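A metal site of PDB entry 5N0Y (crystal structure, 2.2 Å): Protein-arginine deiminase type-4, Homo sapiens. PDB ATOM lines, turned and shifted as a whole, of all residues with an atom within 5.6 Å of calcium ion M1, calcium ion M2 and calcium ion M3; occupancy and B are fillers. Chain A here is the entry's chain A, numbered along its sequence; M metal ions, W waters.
Within 4 Å of calcium ion M2: Asn 160, Asp 162, Asp 164, Asp 172, Asp 183 and Asp 186.
Along chain A the residues within 4 Å of calcium ion M2 span positions 160 to 186.
The nearest printed residue that does not touch calcium ion M2 is Arg 163 (5.1 Å).
The side-chain carboxylate of Asp 395 is in salt-bridge range of the side-chain amino group of Lys 369.
O of Asn 160 is in hydrogen-bond range of SG of Cys 173, 3.2 Å away.
ND2 of Asn 160 lies within hydrogen-bond range of OE1 of Glu 259 (2.8 Å).
Calcium ion M3 is bound by the side-chain carboxylate (OD1) of Asp 175 (2.2 Å).
Calcium ion M3 is bound by the backbone carbonyl oxygen (O) of Glu 177 (2.2 Å).
O of Asp 172 binds calcium ion M3.
Calcium ion M3 is bound by water W1 (2.3 Å).
Calcium ion M3 is bound by water W4 (2.3 Å).
Water W2 is bound to calcium ion M3 (2.4 Å).
Calcium ion M3 has six donor atoms within binding distance.
Calcium ion M2 is bound by the side-chain carboxylate of Asp 172, the side-chain carboxylate of Asp 186, the side-chain carboxylate of Asp 183, the side-chain carboxylate of Asp 162, the side-chain amide oxygen of Asn 160 and the side-chain carboxylate of Asp 164.
Calcium ion M2 has six donor atoms within binding distance.
Within 4 Å of calcium ion M1: Asp 162, Asp 164, Asp 186 and Asp 395.
The nearest printed residue that does not touch calcium ion M1 is Lys 369 (4.6 Å).
The nearest printed residue that does not touch calcium ion M3 is Asp 183 (4.2 Å).
Water W4 lies within hydrogen-bond range of the side-chain carboxylate (OD2) of Asp 183 (2.6 Å), the side-chain carboxylate (OE1) of Glu 259 (2.8 Å) and the side-chain amide nitrogen (ND2) of Asn 160 (3.4 Å).
Water W2 bridges O of Asp 175 and OE2 of Glu 259.
Calcium ion M1 is bound by water W3 (2.2 Å).
Calcium ion M1 is bound by OD1 of Asp 395, 2.3 Å away.
Calcium ion M1 is bound by OD2 of Asp 162.
Calcium ion M1 is bound by OD2 of Asp 164, at 2.5 Å.
OD2 of Asp 186 binds calcium ion M1, 2.5 Å away.
Calcium ion M1 is bound by OD1 of Asp 186 (2.6 Å).
The side-chain carboxylate (OD1) of Asp 164 is bound to calcium ion M1 (2.9 Å).
Calcium ion M1 has seven donor atoms within binding distance.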
ATOM      1  N   ASN A 160     -19.004 -13.379 -17.008  1.00  0.00           N
ATOM      2  CA  ASN A 160     -17.925 -14.265 -16.552  1.00  0.00           C
ATOM      3  C   ASN A 160     -16.640 -13.854 -17.260  1.00  0.00           C
ATOM      4  O   ASN A 160     -16.096 -14.565 -18.082  1.00  0.00           O
ATOM      5  CB  ASN A 160     -18.331 -15.726 -16.774  1.00  0.00           C
ATOM      6  CG  ASN A 160     -17.436 -16.724 -16.048  1.00  0.00           C
ATOM      7  OD1 ASN A 160     -16.608 -16.349 -15.237  1.00  0.00           O
ATOM      8  ND2 ASN A 160     -17.596 -18.000 -16.365  1.00  0.00           N
ATOM      9  N   ASP A 162     -13.695 -12.747 -15.697  1.00  0.00           N
ATOM     10  CA  ASP A 162     -12.395 -13.074 -15.073  1.00  0.00           C
ATOM     11  C   ASP A 162     -11.721 -14.282 -15.776  1.00  0.00           C
ATOM     12  O   ASP A 162     -12.152 -14.722 -16.879  1.00  0.00           O
ATOM     13  CB  ASP A 162     -12.540 -13.249 -13.531  1.00  0.00           C
ATOM     14  CG  ASP A 162     -13.270 -14.522 -13.159  1.00  0.00           C
ATOM     15  OD1 ASP A 162     -13.786 -15.175 -14.091  1.00  0.00           O
ATOM     16  OD2 ASP A 162     -13.363 -14.846 -11.941  1.00  0.00           O
ATOM     17  N   ARG A 163     -10.648 -14.792 -15.150  1.00  0.00           N
ATOM     18  CA  ARG A 163      -9.855 -15.937 -15.666  1.00  0.00           C
ATOM     19  C   ARG A 163      -9.422 -16.790 -14.473  1.00  0.00           C
ATOM     20  O   ARG A 163      -8.286 -16.704 -13.996  1.00  0.00           O
ATOM     21  CB  ARG A 163      -8.682 -15.442 -16.481  1.00  0.00           C
ATOM     22  CG  ARG A 163      -7.600 -16.449 -16.841  1.00  0.00           C
ATOM     23  CD  ARG A 163      -6.541 -15.805 -17.731  1.00  0.00           C
ATOM     24  NE  ARG A 163      -5.689 -14.777 -17.066  1.00  0.00           N
ATOM     25  CZ  ARG A 163      -5.182 -13.677 -17.663  1.00  0.00           C
ATOM     26  NH1 ARG A 163      -5.398 -13.397 -18.950  1.00  0.00           N
ATOM     27  NH2 ARG A 163      -4.448 -12.808 -16.967  1.00  0.00           N
ATOM     28  N   ASP A 164     -10.391 -17.556 -13.951  1.00  0.00           N
ATOM     29  CA  ASP A 164     -10.137 -18.642 -13.006  1.00  0.00           C
ATOM     30  C   ASP A 164      -9.214 -19.773 -13.593  1.00  0.00           C
ATOM     31  O   ASP A 164      -8.518 -20.460 -12.836  1.00  0.00           O
ATOM     32  CB  ASP A 164     -11.448 -19.247 -12.526  1.00  0.00           C
ATOM     33  CG  ASP A 164     -12.221 -18.332 -11.625  1.00  0.00           C
ATOM     34  OD1 ASP A 164     -11.648 -17.797 -10.648  1.00  0.00           O
ATOM     35  OD2 ASP A 164     -13.439 -18.173 -11.859  1.00  0.00           O
ATOM     36  N   ASP A 172     -12.826 -16.570 -18.956  1.00  0.00           N
ATOM     37  CA  ASP A 172     -13.568 -17.851 -18.859  1.00  0.00           C
ATOM     38  C   ASP A 172     -14.700 -18.058 -19.869  1.00  0.00           C
ATOM     39  O   ASP A 172     -14.877 -19.190 -20.353  1.00  0.00           O
ATOM     40  CB  ASP A 172     -14.118 -18.034 -17.450  1.00  0.00           C
ATOM     41  CG  ASP A 172     -13.041 -18.116 -16.420  1.00  0.00           C
ATOM     42  OD1 ASP A 172     -11.854 -18.447 -16.761  1.00  0.00           O
ATOM     43  OD2 ASP A 172     -13.391 -17.872 -15.249  1.00  0.00           O
ATOM     44  N   CYS A 173     -15.445 -16.987 -20.199  1.00  0.00           N
ATOM     45  CA  CYS A 173     -16.677 -17.092 -21.004  1.00  0.00           C
ATOM     46  C   CYS A 173     -16.441 -17.080 -22.526  1.00  0.00           C
ATOM     47  O   CYS A 173     -17.413 -17.101 -23.315  1.00  0.00           O
ATOM     48  CB  CYS A 173     -17.622 -15.944 -20.642  1.00  0.00           C
ATOM     49  SG  CYS A 173     -17.039 -14.284 -21.099  1.00  0.00           S
ATOM     50  N   GLU A 174     -15.174 -17.003 -22.956  1.00  0.00           N
ATOM     51  CA  GLU A 174     -14.902 -17.068 -24.410  1.00  0.00           C
ATOM     52  C   GLU A 174     -14.995 -18.489 -25.080  1.00  0.00           C
ATOM     53  O   GLU A 174     -15.199 -18.577 -26.254  1.00  0.00           O
ATOM     54  CB  GLU A 174     -13.637 -16.286 -24.756  1.00  0.00           C
ATOM     55  CG  GLU A 174     -13.943 -14.781 -24.820  1.00  0.00           C
ATOM     56  CD  GLU A 174     -12.752 -13.851 -24.685  1.00  0.00           C
ATOM     57  OE1 GLU A 174     -11.647 -14.331 -24.337  1.00  0.00           O
ATOM     58  OE2 GLU A 174     -12.904 -12.630 -24.932  1.00  0.00           O
ATOM     59  N   ASP A 175     -14.950 -19.573 -24.337  1.00  0.00           N
ATOM     60  CA  ASP A 175     -15.040 -20.919 -24.921  1.00  0.00           C
ATOM     61  C   ASP A 175     -16.434 -21.461 -24.585  1.00  0.00           C
ATOM     62  O   ASP A 175     -17.233 -20.751 -23.948  1.00  0.00           O
ATOM     63  CB  ASP A 175     -13.924 -21.830 -24.347  1.00  0.00           C
ATOM     64  CG  ASP A 175     -14.083 -22.095 -22.841  1.00  0.00           C
ATOM     65  OD1 ASP A 175     -15.095 -21.647 -22.232  1.00  0.00           O
ATOM     66  OD2 ASP A 175     -13.175 -22.735 -22.244  1.00  0.00           O
ATOM     67  N   ASP A 176     -16.686 -22.725 -24.982  1.00  0.00           N
ATOM     68  CA  ASP A 176     -17.944 -23.457 -24.698  1.00  0.00           C
ATOM     69  C   ASP A 176     -17.833 -24.542 -23.618  1.00  0.00           C
ATOM     70  O   ASP A 176     -18.536 -25.550 -23.696  1.00  0.00           O
ATOM     71  CB  ASP A 176     -18.496 -24.066 -25.996  1.00  0.00           C
ATOM     72  CG  ASP A 176     -18.867 -23.011 -27.041  1.00  0.00           C
ATOM     73  OD1 ASP A 176     -19.889 -22.294 -26.887  1.00  0.00           O
ATOM     74  OD2 ASP A 176     -18.132 -22.907 -28.043  1.00  0.00           O
ATOM     75  N   GLU A 177     -16.988 -24.334 -22.606  1.00  0.00           N
ATOM     76  CA  GLU A 177     -16.778 -25.318 -21.530  1.00  0.00           C
ATOM     77  C   GLU A 177     -16.515 -24.664 -20.166  1.00  0.00           C
ATOM     78  O   GLU A 177     -16.000 -23.532 -20.097  1.00  0.00           O
ATOM     79  CB  GLU A 177     -15.567 -26.256 -21.818  1.00  0.00           C
ATOM     80  CG  GLU A 177     -15.206 -26.483 -23.280  1.00  0.00           C
ATOM     81  CD  GLU A 177     -14.059 -27.462 -23.487  1.00  0.00           C
ATOM     82  OE1 GLU A 177     -13.995 -28.509 -22.808  1.00  0.00           O
ATOM     83  OE2 GLU A 177     -13.214 -27.185 -24.372  1.00  0.00           O
ATOM     84  N   VAL A 178     -16.819 -25.422 -19.107  1.00  0.00           N
ATOM     85  CA  VAL A 178     -16.466 -25.112 -17.733  1.00  0.00           C
ATOM     86  C   VAL A 178     -15.232 -25.928 -17.411  1.00  0.00           C
ATOM     87  O   VAL A 178     -15.347 -27.135 -17.164  1.00  0.00           O
ATOM     88  CB  VAL A 178     -17.562 -25.549 -16.752  1.00  0.00           C
ATOM     89  CG1 VAL A 178     -17.191 -25.225 -15.301  1.00  0.00           C
ATOM     90  CG2 VAL A 178     -18.890 -24.932 -17.142  1.00  0.00           C
ATOM     91  N   LEU A 179     -14.069 -25.277 -17.386  1.00  0.00           N
ATOM     92  CA  LEU A 179     -12.778 -25.955 -17.221  1.00  0.00           C
ATOM     93  C   LEU A 179     -12.287 -26.092 -15.792  1.00  0.00           C
ATOM     94  O   LEU A 179     -11.427 -26.897 -15.570  1.00  0.00           O
ATOM     95  CB  LEU A 179     -11.699 -25.232 -18.026  1.00  0.00           C
ATOM     96  CG  LEU A 179     -11.881 -25.308 -19.533  1.00  0.00           C
ATOM     97  CD1 LEU A 179     -10.772 -24.489 -20.183  1.00  0.00           C
ATOM     98  CD2 LEU A 179     -11.889 -26.750 -20.032  1.00  0.00           C
ATOM     99  N   GLU A 182     -14.225 -24.078  -9.700  1.00  0.00           N
ATOM    100  CA  GLU A 182     -14.271 -22.723  -9.165  1.00  0.00           C
ATOM    101  C   GLU A 182     -15.084 -21.779 -10.074  1.00  0.00           C
ATOM    102  O   GLU A 182     -15.844 -20.967  -9.572  1.00  0.00           O
ATOM    103  CB  GLU A 182     -12.843 -22.150  -9.028  1.00  0.00           C
ATOM    104  CG  GLU A 182     -11.982 -22.705  -7.881  1.00  0.00           C
ATOM    105  CD  GLU A 182     -11.215 -23.990  -8.215  1.00  0.00           C
ATOM    106  OE1 GLU A 182     -10.777 -24.632  -7.244  1.00  0.00           O
ATOM    107  OE2 GLU A 182     -11.056 -24.375  -9.406  1.00  0.00           O
ATOM    108  N   ASP A 183     -14.896 -21.908 -11.390  1.00  0.00           N
ATOM    109  CA  ASP A 183     -15.613 -21.138 -12.392  1.00  0.00           C
ATOM    110  C   ASP A 183     -17.112 -21.107 -12.096  1.00  0.00           C
ATOM    111  O   ASP A 183     -17.728 -20.030 -12.214  1.00  0.00           O
ATOM    112  CB  ASP A 183     -15.349 -21.671 -13.811  1.00  0.00           C
ATOM    113  CG  ASP A 183     -15.775 -20.691 -14.918  1.00  0.00           C
ATOM    114  OD1 ASP A 183     -15.669 -19.480 -14.719  1.00  0.00           O
ATOM    115  OD2 ASP A 183     -16.156 -21.161 -16.024  1.00  0.00           O
ATOM    116  N   ASP A 186     -18.903 -18.265 -10.150  1.00  0.00           N
ATOM    117  CA  ASP A 186     -19.225 -17.056 -10.869  1.00  0.00           C
ATOM    118  C   ASP A 186     -20.611 -17.113 -11.509  1.00  0.00           C
ATOM    119  O   ASP A 186     -21.189 -16.073 -11.785  1.00  0.00           O
ATOM    120  CB  ASP A 186     -18.177 -16.772 -11.935  1.00  0.00           C
ATOM    121  CG  ASP A 186     -16.808 -16.548 -11.362  1.00  0.00           C
ATOM    122  OD1 ASP A 186     -16.687 -16.055 -10.213  1.00  0.00           O
ATOM    123  OD2 ASP A 186     -15.828 -16.867 -12.066  1.00  0.00           O
ATOM    124  N   PHE A 221     -25.192 -24.049 -19.039  1.00  0.00           N
ATOM    125  CA  PHE A 221     -24.599 -25.372 -18.889  1.00  0.00           C
ATOM    126  C   PHE A 221     -25.499 -26.280 -18.104  1.00  0.00           C
ATOM    127  O   PHE A 221     -26.030 -25.852 -17.061  1.00  0.00           O
ATOM    128  CB  PHE A 221     -23.293 -25.285 -18.124  1.00  0.00           C
ATOM    129  CG  PHE A 221     -22.208 -24.596 -18.873  1.00  0.00           C
ATOM    130  CD1 PHE A 221     -21.445 -25.304 -19.834  1.00  0.00           C
ATOM    131  CD2 PHE A 221     -21.913 -23.253 -18.611  1.00  0.00           C
ATOM    132  CE1 PHE A 221     -20.404 -24.662 -20.511  1.00  0.00           C
ATOM    133  CE2 PHE A 221     -20.907 -22.619 -19.315  1.00  0.00           C
ATOM    134  CZ  PHE A 221     -20.156 -23.323 -20.261  1.00  0.00           C
ATOM    135  N   GLU A 259     -23.979 -18.194 -17.397  1.00  0.00           N
ATOM    136  CA  GLU A 259     -23.026 -17.089 -17.424  1.00  0.00           C
ATOM    137  C   GLU A 259     -23.443 -16.092 -18.503  1.00  0.00           C
ATOM    138  O   GLU A 259     -24.009 -16.481 -19.533  1.00  0.00           O
ATOM    139  CB  GLU A 259     -21.577 -17.594 -17.718  1.00  0.00           C
ATOM    140  CG  GLU A 259     -21.453 -18.394 -19.035  1.00  0.00           C
ATOM    141  CD  GLU A 259     -20.030 -18.900 -19.391  1.00  0.00           C
ATOM    142  OE1 GLU A 259     -19.125 -18.789 -18.525  1.00  0.00           O
ATOM    143  OE2 GLU A 259     -19.818 -19.411 -20.552  1.00  0.00           O
ATOM    144  N   LYS A 369     -21.848 -13.707  -5.397  1.00  0.00           N
ATOM    145  CA  LYS A 369     -20.476 -13.467  -5.858  1.00  0.00           C
ATOM    146  C   LYS A 369     -20.267 -11.987  -6.248  1.00  0.00           C
ATOM    147  O   LYS A 369     -21.096 -11.399  -6.950  1.00  0.00           O
ATOM    148  CB  LYS A 369     -20.157 -14.372  -7.046  1.00  0.00           C
ATOM    149  CG  LYS A 369     -18.837 -14.156  -7.717  1.00  0.00           C
ATOM    150  CD  LYS A 369     -17.667 -14.359  -6.772  1.00  0.00           C
ATOM    151  CE  LYS A 369     -17.290 -15.804  -6.549  1.00  0.00           C
ATOM    152  NZ  LYS A 369     -15.921 -15.858  -5.995  1.00  0.00           N
ATOM    153  N   LEU A 371     -16.921  -9.491  -7.523  1.00  0.00           N
ATOM    154  CA  LEU A 371     -15.527  -9.495  -7.848  1.00  0.00           C
ATOM    155  C   LEU A 371     -15.103  -8.214  -8.572  1.00  0.00           C
ATOM    156  O   LEU A 371     -15.903  -7.583  -9.197  1.00  0.00           O
ATOM    157  CB  LEU A 371     -15.227 -10.711  -8.672  1.00  0.00           C
ATOM    158  CG  LEU A 371     -15.929 -10.804 -10.030  1.00  0.00           C
ATOM    159  CD1 LEU A 371     -14.884 -10.668 -11.105  1.00  0.00           C
ATOM    160  CD2 LEU A 371     -16.657 -12.112 -10.274  1.00  0.00           C
ATOM    161  N   PRO A 394      -7.686 -14.891 -11.568  1.00  0.00           N
ATOM    162  CA  PRO A 394      -8.690 -15.524 -10.716  1.00  0.00           C
ATOM    163  C   PRO A 394      -9.411 -14.501  -9.887  1.00  0.00           C
ATOM    164  O   PRO A 394      -8.785 -13.816  -9.088  1.00  0.00           O
ATOM    165  CB  PRO A 394      -7.858 -16.476  -9.815  1.00  0.00           C
ATOM    166  CG  PRO A 394      -6.558 -16.627 -10.520  1.00  0.00           C
ATOM    167  CD  PRO A 394      -6.323 -15.372 -11.312  1.00  0.00           C
ATOM    168  N   ASP A 395     -10.711 -14.407 -10.061  1.00  0.00           N
ATOM    169  CA  ASP A 395     -11.540 -13.461  -9.284  1.00  0.00           C
ATOM    170  C   ASP A 395     -11.218 -11.981  -9.552  1.00  0.00           C
ATOM    171  O   ASP A 395     -11.489 -11.127  -8.736  1.00  0.00           O
ATOM    172  CB  ASP A 395     -11.565 -13.852  -7.787  1.00  0.00           C
ATOM    173  CG  ASP A 395     -12.539 -14.991  -7.527  1.00  0.00           C
ATOM    174  OD1 ASP A 395     -12.970 -15.612  -8.505  1.00  0.00           O
ATOM    175  OD2 ASP A 395     -12.928 -15.268  -6.370  1.00  0.00           O
HETATM  176 CA    CA M   1     -14.143 -16.448 -10.247  1.00  0.00          CA
HETATM  177 CA    CA M   2     -14.818 -17.383 -13.887  1.00  0.00          CA
HETATM  178 CA    CA M   3     -15.513 -21.375 -20.122  1.00  0.00          CA
HETATM  179  O   HOH W   1     -13.280 -21.681 -19.479  1.00  0.00           O
HETATM  180  O   HOH W   2     -17.394 -20.789 -21.552  1.00  0.00           O
HETATM  181  O   HOH W   3     -14.412 -18.374  -9.217  1.00  0.00           O
HETATM  182  O   HOH W   4     -17.002 -20.637 -18.462  1.00  0.00           O
